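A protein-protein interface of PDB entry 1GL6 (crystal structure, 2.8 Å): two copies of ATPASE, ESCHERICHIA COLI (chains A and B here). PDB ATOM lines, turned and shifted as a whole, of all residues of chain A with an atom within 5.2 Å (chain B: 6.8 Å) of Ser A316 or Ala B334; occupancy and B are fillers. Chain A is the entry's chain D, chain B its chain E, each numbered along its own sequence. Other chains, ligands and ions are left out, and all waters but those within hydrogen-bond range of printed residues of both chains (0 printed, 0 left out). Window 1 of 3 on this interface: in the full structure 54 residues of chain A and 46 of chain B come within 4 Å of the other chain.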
ATOM      1  N   ASN A  58       0.347 -22.548 -25.999  1.00  0.00           N
ATOM      2  CA  ASN A  58      -0.923 -23.124 -25.599  1.00  0.00           C
ATOM      3  C   ASN A  58      -1.423 -22.464 -24.323  1.00  0.00           C
ATOM      4  O   ASN A  58      -0.660 -22.270 -23.395  1.00  0.00           O
ATOM      5  CB  ASN A  58      -0.746 -24.614 -25.382  1.00  0.00           C
ATOM      6  CG  ASN A  58      -2.050 -25.346 -25.234  1.00  0.00           C
ATOM      7  OD1 ASN A  58      -2.776 -25.556 -26.202  1.00  0.00           O
ATOM      8  ND2 ASN A  58      -2.362 -25.739 -24.013  1.00  0.00           N
ATOM      9  N   LEU A 314      -2.856 -21.888 -29.513  1.00  0.00           N
ATOM     10  CA  LEU A 314      -3.842 -22.970 -29.389  1.00  0.00           C
ATOM     11  C   LEU A 314      -4.469 -22.858 -27.996  1.00  0.00           C
ATOM     12  O   LEU A 314      -3.941 -22.141 -27.139  1.00  0.00           O
ATOM     13  CB  LEU A 314      -3.146 -24.321 -29.527  1.00  0.00           C
ATOM     14  CG  LEU A 314      -3.167 -25.143 -30.813  1.00  0.00           C
ATOM     15  CD1 LEU A 314      -3.491 -24.284 -32.001  1.00  0.00           C
ATOM     16  CD2 LEU A 314      -1.821 -25.799 -30.959  1.00  0.00           C
ATOM     17  N   GLN A 315      -5.592 -23.550 -27.779  1.00  0.00           N
ATOM     18  CA  GLN A 315      -6.260 -23.545 -26.475  1.00  0.00           C
ATOM     19  C   GLN A 315      -6.468 -24.987 -26.019  1.00  0.00           C
ATOM     20  O   GLN A 315      -5.897 -25.424 -25.017  1.00  0.00           O
ATOM     21  CB  GLN A 315      -7.626 -22.840 -26.521  1.00  0.00           C
ATOM     22  CG  GLN A 315      -8.233 -22.611 -25.115  1.00  0.00           C
ATOM     23  CD  GLN A 315      -9.768 -22.472 -25.084  1.00  0.00           C
ATOM     24  OE1 GLN A 315     -10.496 -23.379 -25.497  1.00  0.00           O
ATOM     25  NE2 GLN A 315     -10.257 -21.342 -24.570  1.00  0.00           N
ATOM     26  N   SER A 316      -7.289 -25.723 -26.757  1.00  0.00           N
ATOM     27  CA  SER A 316      -7.583 -27.117 -26.436  1.00  0.00           C
ATOM     28  C   SER A 316      -7.096 -28.019 -27.573  1.00  0.00           C
ATOM     29  O   SER A 316      -7.231 -27.665 -28.744  1.00  0.00           O
ATOM     30  CB  SER A 316      -9.090 -27.303 -26.217  1.00  0.00           C
ATOM     31  OG  SER A 316      -9.566 -26.453 -25.191  1.00  0.00           O
ATOM     32  N   THR A 317      -6.527 -29.176 -27.227  1.00  0.00           N
ATOM     33  CA  THR A 317      -6.018 -30.109 -28.240  1.00  0.00           C
ATOM     34  C   THR A 317      -7.125 -30.601 -29.192  1.00  0.00           C
ATOM     35  O   THR A 317      -6.856 -31.053 -30.306  1.00  0.00           O
ATOM     36  CB  THR A 317      -5.293 -31.337 -27.574  1.00  0.00           C
ATOM     37  OG1 THR A 317      -6.085 -31.845 -26.496  1.00  0.00           O
ATOM     38  CG2 THR A 317      -3.909 -30.929 -27.025  1.00  0.00           C
ATOM     39  N   SER A 318      -8.371 -30.484 -28.746  1.00  0.00           N
ATOM     40  CA  SER A 318      -9.518 -30.913 -29.522  1.00  0.00           C
ATOM     41  C   SER A 318      -9.833 -29.952 -30.667  1.00  0.00           C
ATOM     42  O   SER A 318     -10.439 -30.333 -31.675  1.00  0.00           O
ATOM     43  CB  SER A 318     -10.730 -31.056 -28.607  1.00  0.00           C
ATOM     44  OG  SER A 318     -10.980 -29.844 -27.922  1.00  0.00           O
ATOM     45  N   GLN A 319      -9.423 -28.700 -30.513  1.00  0.00           N
ATOM     46  CA  GLN A 319      -9.660 -27.716 -31.562  1.00  0.00           C
ATOM     47  C   GLN A 319      -8.932 -28.117 -32.832  1.00  0.00           C
ATOM     48  O   GLN A 319      -9.559 -28.390 -33.848  1.00  0.00           O
ATOM     49  CB  GLN A 319      -9.169 -26.337 -31.131  1.00  0.00           C
ATOM     50  CG  GLN A 319      -9.908 -25.755 -29.935  1.00  0.00           C
ATOM     51  CD  GLN A 319      -9.308 -24.446 -29.466  1.00  0.00           C
ATOM     52  OE1 GLN A 319      -8.080 -24.260 -29.524  1.00  0.00           O
ATOM     53  NE2 GLN A 319     -10.158 -23.539 -28.979  1.00  0.00           N
ATOM     54  N   LEU A 320      -7.605 -28.143 -32.773  1.00  0.00           N
ATOM     55  CA  LEU A 320      -6.808 -28.507 -33.937  1.00  0.00           C
ATOM     56  C   LEU A 320      -7.137 -29.918 -34.411  1.00  0.00           C
ATOM     57  O   LEU A 320      -7.113 -30.200 -35.599  1.00  0.00           O
ATOM     58  CB  LEU A 320      -5.336 -28.433 -33.598  1.00  0.00           C
ATOM     59  CG  LEU A 320      -4.422 -28.382 -34.815  1.00  0.00           C
ATOM     60  CD1 LEU A 320      -4.556 -27.022 -35.453  1.00  0.00           C
ATOM     61  CD2 LEU A 320      -2.989 -28.651 -34.424  1.00  0.00           C
ATOM     62  N   SER A 345      -8.299 -24.279 -18.521  1.00  0.00           N
ATOM     63  CA  SER A 345      -9.418 -24.423 -17.623  1.00  0.00           C
ATOM     64  C   SER A 345      -9.369 -25.782 -16.953  1.00  0.00           C
ATOM     65  O   SER A 345      -8.825 -26.730 -17.521  1.00  0.00           O
ATOM     66  CB  SER A 345     -10.717 -24.258 -18.408  1.00  0.00           C
ATOM     67  OG  SER A 345     -11.834 -24.147 -17.535  1.00  0.00           O
ATOM     68  N   THR A 347     -11.782 -27.491 -16.578  1.00  0.00           N
ATOM     69  CA  THR A 347     -12.856 -28.218 -17.264  1.00  0.00           C
ATOM     70  C   THR A 347     -12.318 -28.906 -18.521  1.00  0.00           C
ATOM     71  O   THR A 347     -13.064 -29.543 -19.263  1.00  0.00           O
ATOM     72  CB  THR A 347     -14.018 -27.285 -17.687  1.00  0.00           C
ATOM     73  OG1 THR A 347     -13.561 -26.397 -18.706  1.00  0.00           O
ATOM     74  CG2 THR A 347     -14.522 -26.470 -16.524  1.00  0.00           C
ATOM     75  N   ASP A 348     -11.017 -28.779 -18.749  1.00  0.00           N
ATOM     76  CA  ASP A 348     -10.386 -29.427 -19.893  1.00  0.00           C
ATOM     77  C   ASP A 348      -9.213 -30.283 -19.418  1.00  0.00           C
ATOM     78  O   ASP A 348      -8.058 -30.075 -19.818  1.00  0.00           O
ATOM     79  CB  ASP A 348      -9.885 -28.390 -20.886  1.00  0.00           C
ATOM     80  CG  ASP A 348      -9.326 -29.015 -22.137  1.00  0.00           C
ATOM     81  OD1 ASP A 348      -9.431 -30.248 -22.273  1.00  0.00           O
ATOM     82  OD2 ASP A 348      -8.788 -28.276 -22.984  1.00  0.00           O
ATOM     83  N   THR A 351      -6.620 -31.684 -22.127  1.00  0.00           N
ATOM     84  CA  THR A 351      -5.579 -30.838 -22.673  1.00  0.00           C
ATOM     85  C   THR A 351      -4.526 -30.557 -21.620  1.00  0.00           C
ATOM     86  O   THR A 351      -3.355 -30.450 -21.947  1.00  0.00           O
ATOM     87  CB  THR A 351      -6.154 -29.509 -23.200  1.00  0.00           C
ATOM     88  OG1 THR A 351      -6.992 -29.771 -24.334  1.00  0.00           O
ATOM     89  CG2 THR A 351      -5.041 -28.572 -23.613  1.00  0.00           C
ATOM     90  N   LEU B  56     -19.493 -23.048 -15.592  1.00  0.00           N
ATOM     91  CA  LEU B  56     -20.198 -24.264 -15.942  1.00  0.00           C
ATOM     92  C   LEU B  56     -20.678 -24.928 -14.652  1.00  0.00           C
ATOM     93  O   LEU B  56     -19.884 -25.173 -13.740  1.00  0.00           O
ATOM     94  CB  LEU B  56     -19.263 -25.192 -16.695  1.00  0.00           C
ATOM     95  CG  LEU B  56     -19.864 -26.412 -17.380  1.00  0.00           C
ATOM     96  CD1 LEU B  56     -20.982 -26.006 -18.281  1.00  0.00           C
ATOM     97  CD2 LEU B  56     -18.789 -27.105 -18.174  1.00  0.00           C
ATOM     98  N   LYS B 327     -14.903 -34.189 -29.763  1.00  0.00           N
ATOM     99  CA  LYS B 327     -13.872 -33.169 -29.951  1.00  0.00           C
ATOM    100  C   LYS B 327     -14.419 -31.771 -29.706  1.00  0.00           C
ATOM    101  O   LYS B 327     -13.873 -31.000 -28.929  1.00  0.00           O
ATOM    102  CB  LYS B 327     -13.270 -33.240 -31.371  1.00  0.00           C
ATOM    103  CG  LYS B 327     -12.288 -34.388 -31.625  1.00  0.00           C
ATOM    104  CD  LYS B 327     -11.189 -34.424 -30.541  1.00  0.00           C
ATOM    105  CE  LYS B 327     -10.233 -35.629 -30.670  1.00  0.00           C
ATOM    106  NZ  LYS B 327      -9.178 -35.644 -29.602  1.00  0.00           N
ATOM    107  N   ALA B 329     -17.169 -30.923 -28.196  1.00  0.00           N
ATOM    108  CA  ALA B 329     -17.721 -30.819 -26.848  1.00  0.00           C
ATOM    109  C   ALA B 329     -16.627 -30.509 -25.824  1.00  0.00           C
ATOM    110  O   ALA B 329     -16.865 -29.771 -24.871  1.00  0.00           O
ATOM    111  CB  ALA B 329     -18.439 -32.104 -26.475  1.00  0.00           C
ATOM    112  N   GLN B 330     -15.441 -31.095 -26.019  1.00  0.00           N
ATOM    113  CA  GLN B 330     -14.280 -30.877 -25.149  1.00  0.00           C
ATOM    114  C   GLN B 330     -13.851 -29.415 -25.207  1.00  0.00           C
ATOM    115  O   GLN B 330     -13.559 -28.793 -24.184  1.00  0.00           O
ATOM    116  CB  GLN B 330     -13.101 -31.739 -25.611  1.00  0.00           C
ATOM    117  CG  GLN B 330     -11.809 -31.525 -24.804  1.00  0.00           C
ATOM    118  CD  GLN B 330     -10.580 -32.171 -25.434  1.00  0.00           C
ATOM    119  OE1 GLN B 330     -10.651 -33.289 -25.949  1.00  0.00           O
ATOM    120  NE2 GLN B 330      -9.440 -31.478 -25.370  1.00  0.00           N
ATOM    121  N   THR B 331     -13.785 -28.896 -26.428  1.00  0.00           N
ATOM    122  CA  THR B 331     -13.405 -27.520 -26.691  1.00  0.00           C
ATOM    123  C   THR B 331     -14.394 -26.597 -26.001  1.00  0.00           C
ATOM    124  O   THR B 331     -14.018 -25.618 -25.356  1.00  0.00           O
ATOM    125  CB  THR B 331     -13.443 -27.232 -28.198  1.00  0.00           C
ATOM    126  OG1 THR B 331     -12.458 -28.026 -28.865  1.00  0.00           O
ATOM    127  CG2 THR B 331     -13.197 -25.763 -28.467  1.00  0.00           C
ATOM    128  N   LEU B 332     -15.668 -26.931 -26.128  1.00  0.00           N
ATOM    129  CA  LEU B 332     -16.713 -26.132 -25.548  1.00  0.00           C
ATOM    130  C   LEU B 332     -16.625 -26.074 -24.028  1.00  0.00           C
ATOM    131  O   LEU B 332     -16.600 -24.992 -23.464  1.00  0.00           O
ATOM    132  CB  LEU B 332     -18.055 -26.681 -25.990  1.00  0.00           C
ATOM    133  CG  LEU B 332     -19.176 -25.652 -26.033  1.00  0.00           C
ATOM    134  CD1 LEU B 332     -18.753 -24.482 -26.896  1.00  0.00           C
ATOM    135  CD2 LEU B 332     -20.439 -26.308 -26.542  1.00  0.00           C
ATOM    136  N   ARG B 333     -16.578 -27.223 -23.358  1.00  0.00           N
ATOM    137  CA  ARG B 333     -16.473 -27.212 -21.900  1.00  0.00           C
ATOM    138  C   ARG B 333     -15.229 -26.471 -21.467  1.00  0.00           C
ATOM    139  O   ARG B 333     -15.260 -25.696 -20.526  1.00  0.00           O
ATOM    140  CB  ARG B 333     -16.377 -28.617 -21.350  1.00  0.00           C
ATOM    141  CG  ARG B 333     -17.526 -29.494 -21.663  1.00  0.00           C
ATOM    142  CD  ARG B 333     -17.369 -30.754 -20.869  1.00  0.00           C
ATOM    143  NE  ARG B 333     -18.258 -31.786 -21.358  1.00  0.00           N
ATOM    144  CZ  ARG B 333     -17.963 -32.631 -22.335  1.00  0.00           C
ATOM    145  NH1 ARG B 333     -16.780 -32.595 -22.945  1.00  0.00           N
ATOM    146  NH2 ARG B 333     -18.886 -33.494 -22.719  1.00  0.00           N
ATOM    147  N   ALA B 334     -14.130 -26.732 -22.162  1.00  0.00           N
ATOM    148  CA  ALA B 334     -12.847 -26.120 -21.864  1.00  0.00           C
ATOM    149  C   ALA B 334     -12.875 -24.605 -21.905  1.00  0.00           C
ATOM    150  O   ALA B 334     -11.989 -23.962 -21.351  1.00  0.00           O
ATOM    151  CB  ALA B 334     -11.799 -26.641 -22.832  1.00  0.00           C
ATOM    152  N   SER B 335     -13.885 -24.035 -22.554  1.00  0.00           N
ATOM    153  CA  SER B 335     -14.013 -22.582 -22.679  1.00  0.00           C
ATOM    154  C   SER B 335     -14.655 -21.890 -21.468  1.00  0.00           C
ATOM    155  O   SER B 335     -14.724 -20.658 -21.422  1.00  0.00           O
ATOM    156  CB  SER B 335     -14.789 -22.248 -23.953  1.00  0.00           C
ATOM    157  OG  SER B 335     -14.058 -22.686 -25.086  1.00  0.00           O
ATOM    158  N   PHE B 336     -15.116 -22.694 -20.504  1.00  0.00           N
ATOM    159  CA  PHE B 336     -15.717 -22.206 -19.254  1.00  0.00           C
ATOM    160  C   PHE B 336     -14.619 -22.384 -18.202  1.00  0.00           C
ATOM    161  O   PHE B 336     -14.332 -23.513 -17.784  1.00  0.00           O
ATOM    162  CB  PHE B 336     -16.915 -23.055 -18.824  1.00  0.00           C
ATOM    163  CG  PHE B 336     -18.107 -22.924 -19.709  1.00  0.00           C
ATOM    164  CD1 PHE B 336     -18.258 -23.734 -20.825  1.00  0.00           C
ATOM    165  CD2 PHE B 336     -19.093 -21.989 -19.423  1.00  0.00           C
ATOM    166  CE1 PHE B 336     -19.374 -23.620 -21.643  1.00  0.00           C
ATOM    167  CE2 PHE B 336     -20.214 -21.866 -20.237  1.00  0.00           C
ATOM    168  CZ  PHE B 336     -20.352 -22.686 -21.347  1.00  0.00           C
ATOM    169  N   ARG B 337     -14.023 -21.274 -17.773  1.00  0.00           N
ATOM    170  CA  ARG B 337     -12.929 -21.299 -16.814  1.00  0.00           C
ATOM    171  C   ARG B 337     -13.327 -21.615 -15.364  1.00  0.00           C
ATOM    172  O   ARG B 337     -12.519 -22.136 -14.592  1.00  0.00           O
ATOM    173  CB  ARG B 337     -12.173 -19.964 -16.894  1.00  0.00           C
ATOM    174  CG  ARG B 337     -11.699 -19.558 -18.307  1.00  0.00           C
ATOM    175  CD  ARG B 337     -10.567 -20.445 -18.812  1.00  0.00           C
ATOM    176  NE  ARG B 337      -9.419 -20.485 -17.901  1.00  0.00           N
ATOM    177  CZ  ARG B 337      -8.589 -19.467 -17.673  1.00  0.00           C
ATOM    178  NH1 ARG B 337      -8.766 -18.299 -18.291  1.00  0.00           N
ATOM    179  NH2 ARG B 337      -7.573 -19.621 -16.828  1.00  0.00           N
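The backbone carbonyl oxygen of Phe B336 lies within hydrogen-bond range of the side-chain hydroxyl of Ser A345. NE2 of Gln B330 lies within hydrogen-bond range of OG1 of Thr A351 (3.2 Å). OG1 of Thr A347 lies within hydrogen-bond range of O of Arg B333, 2.6 Å away. O of Phe B336 is in hydrogen-bond range of OG1 of Thr A347 (3.1 Å). OG of Ser A318 lies within hydrogen-bond range of OG1 of Thr B331 (2.5 Å). The side-chain hydroxyl of Ser A318 sits at hydrogen-bond distance from the side-chain amide nitrogen of Gln B330, 3.4 Å away. OD1 of Asp A348 sits at hydrogen-bond distance from NE2 of Gln B330. The backbone carbonyl oxygen (O) of Lys B327 sits close to the side-chain hydroxyl (OG) of Ser A318, at 3.3 Å.
The side-chain hydroxyl of Thr A347 is in hydrogen-bond range of the side-chain hydroxyl of Ser A345, at 3.1 Å. The side-chain hydroxyl of Thr A351 lies within hydrogen-bond range of the side-chain carboxylate of Asp A348 (2.7 Å). The backbone NH of Ser A316 lies within hydrogen-bond range of the side-chain amide oxygen of Gln A319 (3.2 Å). The backbone carbonyl oxygen of Lys B327 is in hydrogen-bond range of the side-chain hydroxyl of Thr B331 (3.3 Å). The backbone NH of Thr A317 is in hydrogen-bond range of the side-chain hydroxyl of Thr A351, at 3.0 Å. The side-chain hydroxyl (OG) of Ser B335 lies within hydrogen-bond range of the backbone carbonyl oxygen (O) of Thr B331, 2.9 Å away.
Asn A58 touches none of the printed residues of chain B. Ser A316 touches one residue of chain B. Printed residues of chain B within 4 Å of Gln A319: Thr B331 (3.5 Å). Leu A320 touches none of the printed residues of chain B. Of the printed residues of chain B, Thr A347 touches Arg B333, Ala B334 and Phe B336. Of the printed residues of chain A, Gln B330 touches Thr A317 (3.6 Å), Ser A318 (3.4 Å), Asp A348 (3.3 Å) and Thr A351 (3.2 Å). Of the printed residues of chain A, Thr B331 touches Ser A318 (2.5 Å) and Gln A319 (3.5 Å). Ala B334 touches just these residues of chain A: Ser A316, Ser A345, Thr A347 and Asp A348. Of the printed residues of chain A, Phe B336 touches Ser A345 (2.6 Å) and Thr A347 (3.1 Å). The nearest printed residue of chain B that does not touch Ser A316 is Thr B331 (4.3 Å).
No position is printed for both chains. Of the 16 pairs that touch across the chains among the printed residues, none has its exchanged pair printed and touching as well.
OG of Ser B335 touches OE1 of Gln A315, 3.7 Å away. Ala B334 touches Ser A316 (CB to OG, 3.3 Å). Thr A317 touches Gln B330. Thr B331 touches Gln A319 (OG1 to N, 3.5 Å). Ala B334 touches Ser A345 (O to CB, 3.2 Å). OG of Ser A345 touches CA of Arg B337, at 3.1 Å. Thr A347 touches Ala B334 (OG1 to CA, 3.2 Å). Asp A348 touches Ala B334 (CB to CB, 3.2 Å).
Along chain A the printed residues that touch a printed residue of chain B span positions 315 to 351. Of the 11 printed residues of chain B, 8 touch a printed residue of chain A. Hydrophobic or aromatic side chains of chain B within 4 Å of the printed part of chain A: Ala B334.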
